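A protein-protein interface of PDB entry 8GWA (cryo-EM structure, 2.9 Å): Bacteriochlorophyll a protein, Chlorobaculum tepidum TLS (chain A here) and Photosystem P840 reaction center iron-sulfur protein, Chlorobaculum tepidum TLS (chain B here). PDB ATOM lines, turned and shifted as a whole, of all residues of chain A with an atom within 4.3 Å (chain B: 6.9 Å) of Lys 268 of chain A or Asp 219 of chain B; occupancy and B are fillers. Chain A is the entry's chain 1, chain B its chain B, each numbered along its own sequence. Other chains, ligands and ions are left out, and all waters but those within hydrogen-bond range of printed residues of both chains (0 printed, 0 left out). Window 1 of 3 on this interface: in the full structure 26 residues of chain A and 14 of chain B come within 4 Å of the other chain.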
ATOM      1  N   ALA A  32     -20.500  19.723   6.447  1.00  0.00           N
ATOM      2  CA  ALA A  32     -21.031  21.055   6.715  1.00  0.00           C
ATOM      3  C   ALA A  32     -19.890  21.958   7.150  1.00  0.00           C
ATOM      4  O   ALA A  32     -19.238  21.686   8.163  1.00  0.00           O
ATOM      5  CB  ALA A  32     -22.115  21.003   7.787  1.00  0.00           C
ATOM      6  N   ARG A  33     -19.651  23.020   6.391  1.00  0.00           N
ATOM      7  CA  ARG A  33     -18.689  24.047   6.747  1.00  0.00           C
ATOM      8  C   ARG A  33     -19.443  25.313   7.117  1.00  0.00           C
ATOM      9  O   ARG A  33     -20.493  25.614   6.544  1.00  0.00           O
ATOM     10  CB  ARG A  33     -17.716  24.333   5.599  1.00  0.00           C
ATOM     11  CG  ARG A  33     -16.380  23.624   5.721  1.00  0.00           C
ATOM     12  CD  ARG A  33     -16.559  22.122   5.824  1.00  0.00           C
ATOM     13  NE  ARG A  33     -15.361  21.397   5.423  1.00  0.00           N
ATOM     14  CZ  ARG A  33     -15.342  20.112   5.095  1.00  0.00           C
ATOM     15  NH1 ARG A  33     -16.445  19.383   5.100  1.00  0.00           N
ATOM     16  NH2 ARG A  33     -14.189  19.547   4.750  1.00  0.00           N
ATOM     17  N   ALA A 256     -15.463  15.978  12.922  1.00  0.00           N
ATOM     18  CA  ALA A 256     -15.904  17.356  13.037  1.00  0.00           C
ATOM     19  C   ALA A 256     -14.861  18.139  13.816  1.00  0.00           C
ATOM     20  O   ALA A 256     -13.840  17.602  14.251  1.00  0.00           O
ATOM     21  CB  ALA A 256     -17.275  17.459  13.715  1.00  0.00           C
ATOM     22  N   GLY A 257     -15.122  19.428  13.978  1.00  0.00           N
ATOM     23  CA  GLY A 257     -14.228  20.277  14.731  1.00  0.00           C
ATOM     24  C   GLY A 257     -14.545  21.734  14.502  1.00  0.00           C
ATOM     25  O   GLY A 257     -14.856  22.138  13.378  1.00  0.00           O
ATOM     26  N   VAL A 267     -16.363  26.286  11.640  1.00  0.00           N
ATOM     27  CA  VAL A 267     -16.879  24.938  11.845  1.00  0.00           C
ATOM     28  C   VAL A 267     -16.553  24.085  10.628  1.00  0.00           C
ATOM     29  O   VAL A 267     -16.789  24.502   9.490  1.00  0.00           O
ATOM     30  CB  VAL A 267     -18.401  24.942  12.090  1.00  0.00           C
ATOM     31  CG1 VAL A 267     -18.875  23.563  12.525  1.00  0.00           C
ATOM     32  CG2 VAL A 267     -18.778  25.997  13.113  1.00  0.00           C
ATOM     33  N   LYS A 268     -16.015  22.891  10.871  1.00  0.00           N
ATOM     34  CA  LYS A 268     -15.937  21.840   9.866  1.00  0.00           C
ATOM     35  C   LYS A 268     -16.662  20.607  10.379  1.00  0.00           C
ATOM     36  O   LYS A 268     -16.508  20.229  11.545  1.00  0.00           O
ATOM     37  CB  LYS A 268     -14.496  21.456   9.525  1.00  0.00           C
ATOM     38  CG  LYS A 268     -13.549  22.599   9.264  1.00  0.00           C
ATOM     39  CD  LYS A 268     -12.173  22.048   8.932  1.00  0.00           C
ATOM     40  CE  LYS A 268     -11.681  21.113  10.023  1.00  0.00           C
ATOM     41  NZ  LYS A 268     -10.280  20.673   9.794  1.00  0.00           N
ATOM     42  N   VAL A 269     -17.452  19.986   9.509  1.00  0.00           N
ATOM     43  CA  VAL A 269     -18.117  18.725   9.816  1.00  0.00           C
ATOM     44  C   VAL A 269     -17.993  17.823   8.597  1.00  0.00           C
ATOM     45  O   VAL A 269     -18.328  18.237   7.484  1.00  0.00           O
ATOM     46  CB  VAL A 269     -19.596  18.921  10.193  1.00  0.00           C
ATOM     47  CG1 VAL A 269     -20.363  17.617  10.041  1.00  0.00           C
ATOM     48  CG2 VAL A 269     -19.713  19.444  11.613  1.00  0.00           C
ATOM     49  N   ASP B 217      -5.618  24.778  15.079  1.00  0.00           N
ATOM     50  CA  ASP B 217      -5.798  25.460  13.807  1.00  0.00           C
ATOM     51  C   ASP B 217      -6.218  24.469  12.733  1.00  0.00           C
ATOM     52  O   ASP B 217      -5.870  23.286  12.784  1.00  0.00           O
ATOM     53  CB  ASP B 217      -4.513  26.177  13.367  1.00  0.00           C
ATOM     54  CG  ASP B 217      -4.113  27.307  14.304  1.00  0.00           C
ATOM     55  OD1 ASP B 217      -4.838  27.580  15.279  1.00  0.00           O
ATOM     56  OD2 ASP B 217      -3.058  27.930  14.061  1.00  0.00           O
ATOM     57  N   PHE B 218      -6.975  24.972  11.761  1.00  0.00           N
ATOM     58  CA  PHE B 218      -7.283  24.228  10.547  1.00  0.00           C
ATOM     59  C   PHE B 218      -7.628  25.221   9.449  1.00  0.00           C
ATOM     60  O   PHE B 218      -7.879  26.400   9.709  1.00  0.00           O
ATOM     61  CB  PHE B 218      -8.423  23.220  10.754  1.00  0.00           C
ATOM     62  CG  PHE B 218      -9.703  23.821  11.281  1.00  0.00           C
ATOM     63  CD1 PHE B 218     -10.534  24.565  10.458  1.00  0.00           C
ATOM     64  CD2 PHE B 218     -10.097  23.597  12.586  1.00  0.00           C
ATOM     65  CE1 PHE B 218     -11.712  25.100  10.938  1.00  0.00           C
ATOM     66  CE2 PHE B 218     -11.276  24.127  13.069  1.00  0.00           C
ATOM     67  CZ  PHE B 218     -12.084  24.878  12.241  1.00  0.00           C
ATOM     68  N   ASP B 219      -7.640  24.726   8.216  1.00  0.00           N
ATOM     69  CA  ASP B 219      -7.979  25.531   7.049  1.00  0.00           C
ATOM     70  C   ASP B 219      -9.453  25.328   6.727  1.00  0.00           C
ATOM     71  O   ASP B 219      -9.894  24.195   6.505  1.00  0.00           O
ATOM     72  CB  ASP B 219      -7.104  25.153   5.854  1.00  0.00           C
ATOM     73  CG  ASP B 219      -7.069  26.233   4.793  1.00  0.00           C
ATOM     74  OD1 ASP B 219      -6.847  27.410   5.147  1.00  0.00           O
ATOM     75  OD2 ASP B 219      -7.255  25.906   3.602  1.00  0.00           O
ATOM     76  N   LEU B 220     -10.210  26.422   6.703  1.00  0.00           N
ATOM     77  CA  LEU B 220     -11.652  26.370   6.477  1.00  0.00           C
ATOM     78  C   LEU B 220     -11.931  26.604   4.996  1.00  0.00           C
ATOM     79  O   LEU B 220     -11.801  27.727   4.501  1.00  0.00           O
ATOM     80  CB  LEU B 220     -12.370  27.403   7.340  1.00  0.00           C
ATOM     81  CG  LEU B 220     -13.891  27.457   7.192  1.00  0.00           C
ATOM     82  CD1 LEU B 220     -14.507  26.113   7.531  1.00  0.00           C
ATOM     83  CD2 LEU B 220     -14.479  28.551   8.061  1.00  0.00           C
ATOM     84  N   ARG B 221     -12.316  25.543   4.293  1.00  0.00           N
ATOM     85  CA  ARG B 221     -12.665  25.607   2.882  1.00  0.00           C
ATOM     86  C   ARG B 221     -14.106  25.156   2.711  1.00  0.00           C
ATOM     87  O   ARG B 221     -14.488  24.089   3.202  1.00  0.00           O
ATOM     88  CB  ARG B 221     -11.725  24.735   2.048  1.00  0.00           C
ATOM     89  CG  ARG B 221     -10.298  25.251   1.999  1.00  0.00           C
ATOM     90  CD  ARG B 221      -9.303  24.114   1.890  1.00  0.00           C
ATOM     91  NE  ARG B 221      -9.363  23.442   0.599  1.00  0.00           N
ATOM     92  CZ  ARG B 221      -8.427  23.535  -0.336  1.00  0.00           C
ATOM     93  NH1 ARG B 221      -7.358  24.294  -0.170  1.00  0.00           N
ATOM     94  NH2 ARG B 221      -8.568  22.845  -1.463  1.00  0.00           N
ATOM     95  N   HIS B 227     -14.792  28.365  -1.892  1.00  0.00           N
ATOM     96  CA  HIS B 227     -14.002  27.186  -2.201  1.00  0.00           C
ATOM     97  C   HIS B 227     -14.908  26.082  -2.733  1.00  0.00           C
ATOM     98  O   HIS B 227     -16.129  26.221  -2.805  1.00  0.00           O
ATOM     99  CB  HIS B 227     -13.253  26.685  -0.967  1.00  0.00           C
ATOM    100  CG  HIS B 227     -12.113  27.553  -0.555  1.00  0.00           C
ATOM    101  ND1 HIS B 227     -10.901  27.547  -1.210  1.00  0.00           N
ATOM    102  CD2 HIS B 227     -11.994  28.447   0.453  1.00  0.00           C
ATOM    103  CE1 HIS B 227     -10.082  28.399  -0.621  1.00  0.00           C
ATOM    104  NE2 HIS B 227     -10.723  28.959   0.389  1.00  0.00           N
ATOM    105  N   GLU B 229     -13.424  22.709  -1.897  1.00  0.00           N
ATOM    106  CA  GLU B 229     -12.723  21.637  -1.182  1.00  0.00           C
ATOM    107  C   GLU B 229     -12.009  20.764  -2.206  1.00  0.00           C
ATOM    108  O   GLU B 229     -11.204  21.304  -2.985  1.00  0.00           O
ATOM    109  CB  GLU B 229     -13.711  20.915  -0.262  1.00  0.00           C
ATOM    110  CG  GLU B 229     -13.903  21.591   1.085  1.00  0.00           C
ATOM    111  CD  GLU B 229     -12.891  21.141   2.120  1.00  0.00           C
ATOM    112  OE1 GLU B 229     -11.870  20.533   1.736  1.00  0.00           O
ATOM    113  OE2 GLU B 229     -13.115  21.395   3.321  1.00  0.00           O
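Among the printed residues, pairs that only touch across the chains: Arg 33 of chain A with Arg 221 of chain B (3.2 Å), Lys 268 of chain A with Phe 218 of chain B (3.3 Å), Val 267 of chain A with Leu 220 of chain B (3.4 Å), Arg 33 of chain A with Leu 220 of chain B (3.6 Å) and Lys 268 of chain A with Asp 219 of chain B (3.96 Å).
The backbone carbonyl oxygen of Val 269 of chain A lies within hydrogen-bond range of the guanidinium group of Arg 33 of chain A (3.2 Å). O of Gly 257 of chain A is in hydrogen-bond range of N of Lys 268 of chain A (2.9 Å). The backbone carbonyl oxygen (O) of Glu 229 of chain B lies within hydrogen-bond range of the guanidinium group (NH2) of Arg 221 of chain B (3.4 Å).
The side-chain carboxylate (OE2) of Glu 229 of chain B is in salt-bridge range of the guanidinium group (NH2) of Arg 33 of chain A (2.6 Å).
Printed residues of chain B within 4 Å of Lys 268 of chain A: Phe 218 and Asp 219. Of the printed residues of chain A, Asp 219 of chain B touches Lys 268. Of the printed residues of chain A, Glu 229 of chain B touches Arg 33. Of the printed residues of chain A, Phe 218 of chain B touches Lys 268 (3.3 Å). Printed residues of chain B within 4 Å of Arg 33 of chain A: Leu 220 (3.6 Å), Arg 221 (3.2 Å) and Glu 229 (2.6 Å). Of the printed residues of chain A, Arg 221 of chain B touches Arg 33 (3.2 Å). Of the printed residues of chain A, Leu 220 of chain B touches Arg 33 and Val 267. Val 269 of chain A touches none of the printed residues of chain B. The nearest residue of chain B that does not touch Lys 268 of chain A is Leu 220 of chain B (4.03 Å). The nearest printed residue of chain A that does not touch Asp 219 of chain B is Arg 33 of chain A (6.2 Å). The nearest printed residue of chain A that does not touch Leu 220 of chain B is Lys 268 of chain A (4.03 Å).
Of the 7 printed residues of chain B, 5 touch a printed residue of chain A. Printed residues of chain B that touch a printed residue of chain A: Phe 218, Asp 219, Leu 220, Arg 221 and Glu 229. Hydrophobic or aromatic side chains of chain B that line the printed part of chain A: Phe 218 and Leu 220.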
